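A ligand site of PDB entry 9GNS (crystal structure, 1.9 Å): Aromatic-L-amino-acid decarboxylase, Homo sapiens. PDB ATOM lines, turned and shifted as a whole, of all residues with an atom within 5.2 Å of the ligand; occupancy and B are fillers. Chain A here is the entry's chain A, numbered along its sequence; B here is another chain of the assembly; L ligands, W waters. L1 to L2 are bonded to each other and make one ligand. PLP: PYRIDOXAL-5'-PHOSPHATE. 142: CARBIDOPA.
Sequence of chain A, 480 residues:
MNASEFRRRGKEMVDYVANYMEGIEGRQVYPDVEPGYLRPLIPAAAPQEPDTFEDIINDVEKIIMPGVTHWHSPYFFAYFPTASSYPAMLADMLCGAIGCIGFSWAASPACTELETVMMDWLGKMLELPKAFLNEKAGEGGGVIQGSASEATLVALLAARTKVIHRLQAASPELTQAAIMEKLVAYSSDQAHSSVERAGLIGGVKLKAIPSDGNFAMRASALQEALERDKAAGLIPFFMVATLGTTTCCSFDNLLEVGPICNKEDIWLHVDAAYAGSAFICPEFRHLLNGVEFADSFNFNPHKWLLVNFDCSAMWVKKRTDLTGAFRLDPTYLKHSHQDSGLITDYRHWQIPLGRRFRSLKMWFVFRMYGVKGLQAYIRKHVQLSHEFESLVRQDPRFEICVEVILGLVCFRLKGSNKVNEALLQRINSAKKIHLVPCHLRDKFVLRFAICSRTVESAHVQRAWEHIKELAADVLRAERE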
ATOM      1  N   TRP A  71      10.304 -22.344 -23.886  1.00  0.00           N
ATOM      2  CA  TRP A  71      11.238 -21.840 -22.871  1.00  0.00           C
ATOM      3  C   TRP A  71      10.987 -20.389 -22.512  1.00  0.00           C
ATOM      4  O   TRP A  71      11.333 -19.942 -21.406  1.00  0.00           O
ATOM      5  CB  TRP A  71      12.678 -21.955 -23.370  1.00  0.00           C
ATOM      6  CG  TRP A  71      13.275 -23.319 -23.260  1.00  0.00           C
ATOM      7  CD1 TRP A  71      12.963 -24.418 -24.015  1.00  0.00           C
ATOM      8  CD2 TRP A  71      14.272 -23.740 -22.332  1.00  0.00           C
ATOM      9  NE1 TRP A  71      13.727 -25.488 -23.620  1.00  0.00           N
ATOM     10  CE2 TRP A  71      14.536 -25.103 -22.577  1.00  0.00           C
ATOM     11  CE3 TRP A  71      14.973 -23.092 -21.305  1.00  0.00           C
ATOM     12  CZ2 TRP A  71      15.475 -25.832 -21.844  1.00  0.00           C
ATOM     13  CZ3 TRP A  71      15.904 -23.817 -20.573  1.00  0.00           C
ATOM     14  CH2 TRP A  71      16.151 -25.174 -20.848  1.00  0.00           C
ATOM     15  N   TYR A  79      14.150 -25.937 -15.038  1.00  0.00           N
ATOM     16  CA  TYR A  79      15.602 -25.867 -15.190  1.00  0.00           C
ATOM     17  C   TYR A  79      16.156 -24.527 -14.719  1.00  0.00           C
ATOM     18  O   TYR A  79      16.036 -24.166 -13.545  1.00  0.00           O
ATOM     19  CB  TYR A  79      15.991 -26.142 -16.649  1.00  0.00           C
ATOM     20  CG  TYR A  79      15.242 -27.305 -17.280  1.00  0.00           C
ATOM     21  CD1 TYR A  79      15.446 -28.614 -16.843  1.00  0.00           C
ATOM     22  CD2 TYR A  79      14.371 -27.104 -18.351  1.00  0.00           C
ATOM     23  CE1 TYR A  79      14.772 -29.684 -17.423  1.00  0.00           C
ATOM     24  CE2 TYR A  79      13.685 -28.176 -18.938  1.00  0.00           C
ATOM     25  CZ  TYR A  79      13.900 -29.457 -18.460  1.00  0.00           C
ATOM     26  OH  TYR A  79      13.259 -30.526 -19.040  1.00  0.00           O
ATOM     27  N   PHE A  80      16.783 -23.793 -15.632  1.00  0.00           N
ATOM     28  CA  PHE A  80      17.232 -22.432 -15.456  1.00  0.00           C
ATOM     29  C   PHE A  80      16.817 -21.669 -16.712  1.00  0.00           C
ATOM     30  O   PHE A  80      16.586 -22.285 -17.753  1.00  0.00           O
ATOM     31  CB  PHE A  80      18.763 -22.362 -15.280  1.00  0.00           C
ATOM     32  CG  PHE A  80      19.244 -22.618 -13.872  1.00  0.00           C
ATOM     33  CD1 PHE A  80      18.556 -22.131 -12.777  1.00  0.00           C
ATOM     34  CD2 PHE A  80      20.406 -23.342 -13.654  1.00  0.00           C
ATOM     35  CE1 PHE A  80      19.009 -22.367 -11.485  1.00  0.00           C
ATOM     36  CE2 PHE A  80      20.865 -23.589 -12.368  1.00  0.00           C
ATOM     37  CZ  PHE A  80      20.165 -23.104 -11.280  1.00  0.00           C
ATOM     38  N   PRO A  81      16.710 -20.348 -16.645  1.00  0.00           N
ATOM     39  CA  PRO A  81      16.418 -19.603 -17.876  1.00  0.00           C
ATOM     40  C   PRO A  81      17.459 -19.881 -18.952  1.00  0.00           C
ATOM     41  O   PRO A  81      18.627 -20.162 -18.656  1.00  0.00           O
ATOM     42  CB  PRO A  81      16.460 -18.129 -17.427  1.00  0.00           C
ATOM     43  CG  PRO A  81      17.326 -18.135 -16.195  1.00  0.00           C
ATOM     44  CD  PRO A  81      16.991 -19.451 -15.513  1.00  0.00           C
ATOM     45  N   THR A  82      17.019 -19.822 -20.201  1.00  0.00           N
ATOM     46  CA  THR A  82      17.958 -19.619 -21.283  1.00  0.00           C
ATOM     47  C   THR A  82      17.649 -18.274 -21.924  1.00  0.00           C
ATOM     48  O   THR A  82      16.521 -17.764 -21.813  1.00  0.00           O
ATOM     49  CB  THR A  82      17.920 -20.760 -22.326  1.00  0.00           C
ATOM     50  OG1 THR A  82      19.112 -20.691 -23.137  1.00  0.00           O
ATOM     51  CG2 THR A  82      16.720 -20.626 -23.243  1.00  0.00           C
ATOM     52  N   ALA A  83      18.655 -17.686 -22.547  1.00  0.00           N
ATOM     53  CA  ALA A  83      18.578 -16.295 -22.974  1.00  0.00           C
ATOM     54  C   ALA A  83      17.774 -16.141 -24.253  1.00  0.00           C
ATOM     55  O   ALA A  83      17.911 -16.928 -25.200  1.00  0.00           O
ATOM     56  CB  ALA A  83      19.981 -15.726 -23.175  1.00  0.00           C
ATOM     57  N   GLY A 146      31.373 -22.715 -26.321  1.00  0.00           N
ATOM     58  CA  GLY A 146      30.027 -23.058 -26.762  1.00  0.00           C
ATOM     59  C   GLY A 146      29.063 -23.356 -25.630  1.00  0.00           C
ATOM     60  O   GLY A 146      27.849 -23.225 -25.809  1.00  0.00           O
ATOM     61  N   SER A 147      29.582 -23.727 -24.468  1.00  0.00           N
ATOM     62  CA  SER A 147      28.753 -24.161 -23.357  1.00  0.00           C
ATOM     63  C   SER A 147      29.627 -24.265 -22.117  1.00  0.00           C
ATOM     64  O   SER A 147      30.847 -24.394 -22.215  1.00  0.00           O
ATOM     65  CB  SER A 147      28.072 -25.492 -23.675  1.00  0.00           C
ATOM     66  OG  SER A 147      29.004 -26.557 -23.632  1.00  0.00           O
ATOM     67  N   ALA A 148      28.981 -24.194 -20.951  1.00  0.00           N
ATOM     68  CA  ALA A 148      29.713 -24.386 -19.706  1.00  0.00           C
ATOM     69  C   ALA A 148      30.222 -25.818 -19.593  1.00  0.00           C
ATOM     70  O   ALA A 148      31.272 -26.050 -18.977  1.00  0.00           O
ATOM     71  CB  ALA A 148      28.835 -24.027 -18.498  1.00  0.00           C
ATOM     72  N   SER A 149      29.497 -26.783 -20.154  1.00  0.00           N
ATOM     73  CA  SER A 149      29.970 -28.165 -20.152  1.00  0.00           C
ATOM     74  C   SER A 149      31.285 -28.268 -20.882  1.00  0.00           C
ATOM     75  O   SER A 149      32.201 -28.967 -20.443  1.00  0.00           O
ATOM     76  CB  SER A 149      28.936 -29.089 -20.787  1.00  0.00           C
ATOM     77  OG  SER A 149      27.697 -29.043 -20.108  1.00  0.00           O
ATOM     78  N   GLU A 150      31.398 -27.569 -22.015  1.00  0.00           N
ATOM     79  CA  GLU A 150      32.641 -27.568 -22.762  1.00  0.00           C
ATOM     80  C   GLU A 150      33.726 -26.800 -22.000  1.00  0.00           C
ATOM     81  O   GLU A 150      34.888 -27.202 -21.999  1.00  0.00           O
ATOM     82  CB  GLU A 150      32.433 -26.945 -24.144  1.00  0.00           C
ATOM     83  CG  GLU A 150      31.738 -27.875 -25.119  1.00  0.00           C
ATOM     84  CD  GLU A 150      31.067 -27.123 -26.267  1.00  0.00           C
ATOM     85  OE1 GLU A 150      31.721 -27.002 -27.320  1.00  0.00           O
ATOM     86  OE2 GLU A 150      29.926 -26.635 -26.111  1.00  0.00           O
ATOM     87  N   HIS A 192      26.963 -30.189 -11.465  1.00  0.00           N
ATOM     88  CA  HIS A 192      26.252 -30.532 -12.687  1.00  0.00           C
ATOM     89  C   HIS A 192      26.887 -31.749 -13.341  1.00  0.00           C
ATOM     90  O   HIS A 192      28.080 -32.020 -13.187  1.00  0.00           O
ATOM     91  CB  HIS A 192      26.273 -29.329 -13.643  1.00  0.00           C
ATOM     92  CG  HIS A 192      25.436 -29.518 -14.881  1.00  0.00           C
ATOM     93  ND1 HIS A 192      25.980 -29.858 -16.097  1.00  0.00           N
ATOM     94  CD2 HIS A 192      24.102 -29.409 -15.074  1.00  0.00           C
ATOM     95  CE1 HIS A 192      25.016 -29.947 -17.005  1.00  0.00           C
ATOM     96  NE2 HIS A 192      23.870 -29.691 -16.404  1.00  0.00           N
ATOM     97  N   SER A 194      27.881 -32.159 -16.139  1.00  0.00           N
ATOM     98  CA  SER A 194      28.985 -31.817 -17.030  1.00  0.00           C
ATOM     99  C   SER A 194      30.336 -32.115 -16.402  1.00  0.00           C
ATOM    100  O   SER A 194      31.316 -32.362 -17.120  1.00  0.00           O
ATOM    101  CB  SER A 194      28.914 -30.341 -17.429  1.00  0.00           C
ATOM    102  OG  SER A 194      28.757 -29.523 -16.278  1.00  0.00           O
ATOM    103  N   THR A 242      31.302 -24.910  -7.509  1.00  0.00           N
ATOM    104  CA  THR A 242      30.098 -24.425  -8.171  1.00  0.00           C
ATOM    105  C   THR A 242      29.499 -23.258  -7.406  1.00  0.00           C
ATOM    106  O   THR A 242      29.300 -23.335  -6.190  1.00  0.00           O
ATOM    107  CB  THR A 242      29.064 -25.543  -8.315  1.00  0.00           C
ATOM    108  OG1 THR A 242      29.647 -26.665  -8.998  1.00  0.00           O
ATOM    109  CG2 THR A 242      27.832 -25.060  -9.083  1.00  0.00           C
ATOM    110  N   GLY A 244      26.063 -21.498  -7.545  1.00  0.00           N
ATOM    111  CA  GLY A 244      24.727 -21.650  -8.100  1.00  0.00           C
ATOM    112  C   GLY A 244      24.447 -23.047  -8.617  1.00  0.00           C
ATOM    113  O   GLY A 244      24.292 -23.246  -9.824  1.00  0.00           O
ATOM    114  N   THR A 245      24.372 -24.022  -7.709  1.00  0.00           N
ATOM    115  CA  THR A 245      24.235 -25.409  -8.117  1.00  0.00           C
ATOM    116  C   THR A 245      22.917 -25.615  -8.866  1.00  0.00           C
ATOM    117  O   THR A 245      21.917 -24.936  -8.623  1.00  0.00           O
ATOM    118  CB  THR A 245      24.292 -26.348  -6.911  1.00  0.00           C
ATOM    119  OG1 THR A 245      23.301 -25.976  -5.940  1.00  0.00           O
ATOM    120  CG2 THR A 245      25.680 -26.286  -6.269  1.00  0.00           C
ATOM    121  N   THR A 246      22.939 -26.572  -9.795  1.00  0.00           N
ATOM    122  CA  THR A 246      21.768 -26.831 -10.629  1.00  0.00           C
ATOM    123  C   THR A 246      20.589 -27.314  -9.799  1.00  0.00           C
ATOM    124  O   THR A 246      19.428 -27.024 -10.139  1.00  0.00           O
ATOM    125  CB  THR A 246      22.118 -27.862 -11.702  1.00  0.00           C
ATOM    126  OG1 THR A 246      23.441 -27.612 -12.183  1.00  0.00           O
ATOM    127  CG2 THR A 246      21.139 -27.782 -12.872  1.00  0.00           C
ATOM    128  N   ASP A 271      32.683 -22.925 -11.601  1.00  0.00           N
ATOM    129  CA  ASP A 271      31.528 -23.061 -12.481  1.00  0.00           C
ATOM    130  C   ASP A 271      30.391 -22.252 -11.876  1.00  0.00           C
ATOM    131  O   ASP A 271      29.827 -22.631 -10.849  1.00  0.00           O
ATOM    132  CB  ASP A 271      31.168 -24.534 -12.624  1.00  0.00           C
ATOM    133  CG  ASP A 271      29.797 -24.769 -13.258  1.00  0.00           C
ATOM    134  OD1 ASP A 271      29.167 -23.827 -13.774  1.00  0.00           O
ATOM    135  OD2 ASP A 271      29.360 -25.944 -13.271  1.00  0.00           O
ATOM    136  N   ALA A 273      27.661 -21.260 -13.945  1.00  0.00           N
ATOM    137  CA  ALA A 273      26.877 -21.223 -15.185  1.00  0.00           C
ATOM    138  C   ALA A 273      25.670 -20.299 -15.109  1.00  0.00           C
ATOM    139  O   ALA A 273      25.485 -19.422 -15.965  1.00  0.00           O
ATOM    140  CB  ALA A 273      26.434 -22.640 -15.548  1.00  0.00           C
ATOM    141  N   TYR A 274      24.833 -20.485 -14.090  1.00  0.00           N
ATOM    142  CA  TYR A 274      23.612 -19.698 -13.939  1.00  0.00           C
ATOM    143  C   TYR A 274      23.854 -18.436 -13.128  1.00  0.00           C
ATOM    144  O   TYR A 274      23.579 -17.323 -13.587  1.00  0.00           O
ATOM    145  CB  TYR A 274      22.513 -20.546 -13.276  1.00  0.00           C
ATOM    146  CG  TYR A 274      21.374 -19.723 -12.714  1.00  0.00           C
ATOM    147  CD1 TYR A 274      20.503 -19.051 -13.568  1.00  0.00           C
ATOM    148  CD2 TYR A 274      21.185 -19.598 -11.352  1.00  0.00           C
ATOM    149  CE1 TYR A 274      19.450 -18.289 -13.071  1.00  0.00           C
ATOM    150  CE2 TYR A 274      20.149 -18.844 -10.840  1.00  0.00           C
ATOM    151  CZ  TYR A 274      19.282 -18.190 -11.706  1.00  0.00           C
ATOM    152  OH  TYR A 274      18.243 -17.442 -11.200  1.00  0.00           O
ATOM    153  N   ASN A 300      27.488 -18.628 -17.896  1.00  0.00           N
ATOM    154  CA  ASN A 300      26.774 -18.612 -19.175  1.00  0.00           C
ATOM    155  C   ASN A 300      25.957 -17.342 -19.332  1.00  0.00           C
ATOM    156  O   ASN A 300      24.862 -17.238 -18.746  1.00  0.00           O
ATOM    157  CB  ASN A 300      25.844 -19.831 -19.273  1.00  0.00           C
ATOM    158  CG  ASN A 300      26.598 -21.099 -19.530  1.00  0.00           C
ATOM    159  OD1 ASN A 300      27.733 -21.080 -19.990  1.00  0.00           O
ATOM    160  ND2 ASN A 300      25.967 -22.220 -19.211  1.00  0.00           N
ATOM    161  N   HIS A 302      24.382 -17.125 -21.839  1.00  0.00           N
ATOM    162  CA  HIS A 302      23.214 -17.681 -22.514  1.00  0.00           C
ATOM    163  C   HIS A 302      22.210 -18.317 -21.554  1.00  0.00           C
ATOM    164  O   HIS A 302      21.177 -18.821 -22.024  1.00  0.00           O
ATOM    165  CB  HIS A 302      23.626 -18.658 -23.624  1.00  0.00           C
ATOM    166  CG  HIS A 302      24.252 -19.941 -23.173  1.00  0.00           C
ATOM    167  ND1 HIS A 302      25.304 -20.518 -23.848  1.00  0.00           N
ATOM    168  CD2 HIS A 302      23.948 -20.800 -22.166  1.00  0.00           C
ATOM    169  CE1 HIS A 302      25.636 -21.658 -23.266  1.00  0.00           C
ATOM    170  NE2 HIS A 302      24.831 -21.842 -22.232  1.00  0.00           N
ATOM    171  N   LYS A 303      22.450 -18.277 -20.246  1.00  0.00           N
ATOM    172  CA  LYS A 303      21.381 -18.583 -19.286  1.00  0.00           C
ATOM    173  C   LYS A 303      20.703 -17.276 -18.875  1.00  0.00           C
ATOM    174  O   LYS A 303      19.563 -17.014 -19.240  1.00  0.00           O
ATOM    175  CB  LYS A 303      21.927 -19.331 -18.057  1.00  0.00           C
ATOM    176  CG  LYS A 303      22.132 -20.813 -18.272  1.00  0.00           C
ATOM    177  CD  LYS A 303      22.544 -21.484 -16.960  1.00  0.00           C
ATOM    178  CE  LYS A 303      22.621 -22.993 -17.105  1.00  0.00           C
ATOM    179  NZ  LYS A 303      23.421 -23.377 -18.312  1.00  0.00           N
ATOM    180  N   PHE A 309      21.834 -18.512 -26.612  1.00  0.00           N
ATOM    181  CA  PHE A 309      22.696 -19.667 -26.855  1.00  0.00           C
ATOM    182  C   PHE A 309      23.123 -19.725 -28.317  1.00  0.00           C
ATOM    183  O   PHE A 309      22.332 -19.448 -29.215  1.00  0.00           O
ATOM    184  CB  PHE A 309      21.903 -20.933 -26.463  1.00  0.00           C
ATOM    185  CG  PHE A 309      22.720 -22.196 -26.435  1.00  0.00           C
ATOM    186  CD1 PHE A 309      23.008 -22.882 -27.615  1.00  0.00           C
ATOM    187  CD2 PHE A 309      23.146 -22.733 -25.240  1.00  0.00           C
ATOM    188  CE1 PHE A 309      23.737 -24.071 -27.580  1.00  0.00           C
ATOM    189  CE2 PHE A 309      23.888 -23.919 -25.198  1.00  0.00           C
ATOM    190  CZ  PHE A 309      24.175 -24.581 -26.373  1.00  0.00           C
ATOM    191  N   ILE B 101      16.738 -25.224 -25.649  1.00  0.00           N
ATOM    192  CA  ILE B 101      17.987 -25.951 -25.436  1.00  0.00           C
ATOM    193  C   ILE B 101      17.639 -27.428 -25.457  1.00  0.00           C
ATOM    194  O   ILE B 101      17.070 -27.942 -24.484  1.00  0.00           O
ATOM    195  CB  ILE B 101      18.663 -25.553 -24.119  1.00  0.00           C
ATOM    196  CG1 ILE B 101      18.750 -24.030 -24.015  1.00  0.00           C
ATOM    197  CG2 ILE B 101      20.060 -26.194 -24.030  1.00  0.00           C
ATOM    198  CD1 ILE B 101      19.499 -23.374 -25.188  1.00  0.00           C
ATOM    199  N   PHE B 103      18.665 -30.401 -24.739  1.00  0.00           N
ATOM    200  CA  PHE B 103      19.493 -31.395 -24.058  1.00  0.00           C
ATOM    201  C   PHE B 103      18.718 -32.647 -23.675  1.00  0.00           C
ATOM    202  O   PHE B 103      19.299 -33.569 -23.112  1.00  0.00           O
ATOM    203  CB  PHE B 103      20.113 -30.794 -22.796  1.00  0.00           C
ATOM    204  CG  PHE B 103      19.091 -30.212 -21.850  1.00  0.00           C
ATOM    205  CD1 PHE B 103      18.378 -31.042 -20.996  1.00  0.00           C
ATOM    206  CD2 PHE B 103      18.815 -28.861 -21.860  1.00  0.00           C
ATOM    207  CE1 PHE B 103      17.424 -30.515 -20.144  1.00  0.00           C
ATOM    208  CE2 PHE B 103      17.867 -28.345 -21.014  1.00  0.00           C
ATOM    209  CZ  PHE B 103      17.181 -29.165 -20.153  1.00  0.00           C
ATOM    210  N   LEU B 353      26.326 -30.779 -23.608  1.00  0.00           N
ATOM    211  CA  LEU B 353      24.982 -31.223 -23.231  1.00  0.00           C
ATOM    212  C   LEU B 353      23.919 -30.400 -23.931  1.00  0.00           C
ATOM    213  O   LEU B 353      22.957 -30.952 -24.475  1.00  0.00           O
ATOM    214  CB  LEU B 353      24.775 -31.094 -21.713  1.00  0.00           C
ATOM    215  CG  LEU B 353      25.188 -32.173 -20.715  1.00  0.00           C
ATOM    216  CD1 LEU B 353      24.730 -33.564 -21.158  1.00  0.00           C
ATOM    217  CD2 LEU B 353      26.683 -32.105 -20.490  1.00  0.00           C
ATOM    218  N   GLY B 354      24.070 -29.079 -23.901  1.00  0.00           N
ATOM    219  CA  GLY B 354      23.136 -28.215 -24.580  1.00  0.00           C
ATOM    220  C   GLY B 354      23.340 -28.207 -26.074  1.00  0.00           C
ATOM    221  O   GLY B 354      24.414 -28.531 -26.571  1.00  0.00           O
HETATM  222  N1  PLP L   1      27.054 -25.940 -14.549  1.00  0.00           N
HETATM  223  C2  PLP L   1      25.816 -25.701 -14.027  1.00  0.00           C
HETATM  224  C2A PLP L   1      25.678 -25.343 -12.583  1.00  0.00           C
HETATM  225  C3  PLP L   1      24.696 -25.803 -14.837  1.00  0.00           C
HETATM  226  O3  PLP L   1      23.458 -25.562 -14.302  1.00  0.00           O
HETATM  227  C4  PLP L   1      24.839 -26.140 -16.183  1.00  0.00           C
HETATM  228  C4A PLP L   1      23.649 -26.485 -17.025  1.00  0.00           C
HETATM  229  C5  PLP L   1      26.103 -26.390 -16.689  1.00  0.00           C
HETATM  230  C6  PLP L   1      27.214 -26.285 -15.880  1.00  0.00           C
HETATM  231  C5A PLP L   1      26.251 -26.731 -18.156  1.00  0.00           C
HETATM  232  O4P PLP L   1      25.938 -25.573 -18.903  1.00  0.00           O
HETATM  233  P   PLP L   1      25.722 -25.715 -20.492  1.00  0.00           P
HETATM  234  O1P PLP L   1      26.074 -24.407 -21.159  1.00  0.00           O
HETATM  235  O2P PLP L   1      26.664 -26.821 -20.943  1.00  0.00           O
HETATM  236  O3P PLP L   1      24.285 -26.092 -20.797  1.00  0.00           O
HETATM  237  NN  142 L   2      21.586 -27.225 -17.172  1.00  0.00           N
HETATM  238  N   142 L   2      22.316 -26.118 -16.672  1.00  0.00           N
HETATM  239  CA  142 L   2      20.124 -27.120 -16.942  1.00  0.00           C
HETATM  240  CB  142 L   2      19.568 -27.002 -18.383  1.00  0.00           C
HETATM  241  CB1 142 L   2      19.685 -26.051 -15.932  1.00  0.00           C
HETATM  242  CG  142 L   2      19.913 -25.696 -19.121  1.00  0.00           C
HETATM  243  CD1 142 L   2      20.997 -25.673 -19.987  1.00  0.00           C
HETATM  244  CE1 142 L   2      21.322 -24.494 -20.672  1.00  0.00           C
HETATM  245  CD2 142 L   2      19.128 -24.552 -18.961  1.00  0.00           C
HETATM  246  CE2 142 L   2      19.454 -23.374 -19.646  1.00  0.00           C
HETATM  247  CZ  142 L   2      20.558 -23.353 -20.504  1.00  0.00           C
HETATM  248  OH  142 L   2      20.921 -22.148 -21.234  1.00  0.00           O
HETATM  249  OE1 142 L   2      22.452 -24.448 -21.567  1.00  0.00           O
HETATM  250  C   142 L   2      19.759 -28.561 -16.570  1.00  0.00           C
HETATM  251  O   142 L   2      18.578 -28.877 -16.399  1.00  0.00           O
HETATM  252  OXT 142 L   2      20.660 -29.400 -16.419  1.00  0.00           O
HETATM  253  O   HOH W   1      23.225 -28.406 -20.582  1.00  0.00           O
HETATM  254  O   HOH W   2      20.991 -31.046 -14.120  1.00  0.00           O
HETATM  255  O   HOH W   3      26.598 -28.182 -23.047  1.00  0.00           O
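The backbone NH (N) of Ser 149 lies within hydrogen-bond range of an oxygen (O2P) of PLP L1 (2.9 Å). OG1 of Thr 246 is in hydrogen-bond range of O3 of PLP L1 (2.9 Å). OXT of 142 L2 sits at hydrogen-bond distance from NE2 of His 192. An oxygen (O2P) of PLP L1 is in hydrogen-bond range of the side-chain hydroxyl (OG) of Ser 149, at 2.6 Å. O1P of PLP L1 sits at hydrogen-bond distance from ND2 of Asn 300 (2.9 Å). An oxygen (OH) of 142 L2 lies within hydrogen-bond range of the side-chain hydroxyl (OG1) of Thr 82, 3.0 Å away. The backbone carbonyl oxygen of His 302 sits at hydrogen-bond distance from an oxygen (OH) of 142 L2 (3.4 Å). The side-chain amino group (NZ) of Lys 303 lies within salt-bridge range of an oxygen (O3P) of PLP L1, at 3.8 Å. O1P of PLP L1 is in hydrogen-bond range of N of Ala 148 (2.9 Å). The side-chain carboxylate (OD2) of Asp 271 lies within hydrogen-bond range of a nitrogen (N1) of PLP L1, at 2.6 Å. NE2 of His 302 lies within hydrogen-bond range of O1P of PLP L1.
OG of Ser 194 is in hydrogen-bond range of ND1 of His 192 (2.8 Å). The side-chain carboxylate of Glu 150 lies within hydrogen-bond range of the side-chain hydroxyl of Ser 147. N of Ala 83 is in hydrogen-bond range of O of His 302 (2.8 Å). The side-chain carboxylate (OD1) of Asp 271 sits at hydrogen-bond distance from the backbone NH (N) of Ala 273. The backbone carbonyl oxygen (O) of Lys 303 lies within hydrogen-bond range of the backbone NH (N) of Ala 83, at 3.5 Å. NE2 of His 302 is in hydrogen-bond range of ND2 of Asn 300 (3.2 Å). The backbone NH of Asn 300 sits at hydrogen-bond distance from the backbone carbonyl oxygen of Ala 273 (2.9 Å). The backbone carbonyl oxygen (O) of His 302 is in hydrogen-bond range of the side-chain hydroxyl (OG1) of Thr 82 (3.0 Å).
Merely in contact with the ligand: Trp 71 (3.6 Å), Tyr 79 (3.2 Å), Phe 80 (3.6 Å), Pro 81 (3.5 Å), Ser 147 (3.3 Å), Ser 194 (3.6 Å), Gly 244 (3.7 Å), Ala 273 (3.5 Å), Phe 309 (3.9 Å), Ile 101 of chain B (3.9 Å) and Phe 103 of chain B (3.4 Å). Hydrophobic or aromatic side chains within 4 Å of the ligand: Trp 71, Tyr 79, Phe 80, Ala 148, His 192, Ala 273, His 302, Phe 309, Ile 101 of chain B and Phe 103 of chain B. 20 residues have an atom within 4 Å of the ligand: Trp 71, Tyr 79, Phe 80, Pro 81, Thr 82, Ser 147, Ala 148, Ser 149, His 192, Ser 194, Gly 244, Thr 246, Asp 271, Ala 273, Asn 300, His 302, Lys 303, Phe 309, Ile 101 of chain B and Phe 103 of chain B.
Water W3 lies within hydrogen-bond range of O2P of PLP L1 (2.5 Å), N of Leu 353 of chain B (2.7 Å), N of Gly 354 of chain B (2.8 Å), OG of Ser 147 (3.0 Å) and OG of Ser 149 (3.3 Å). Water W1 bridges O3P of PLP L1 (2.6 Å) and N of Gly 354 of chain B (3.5 Å).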
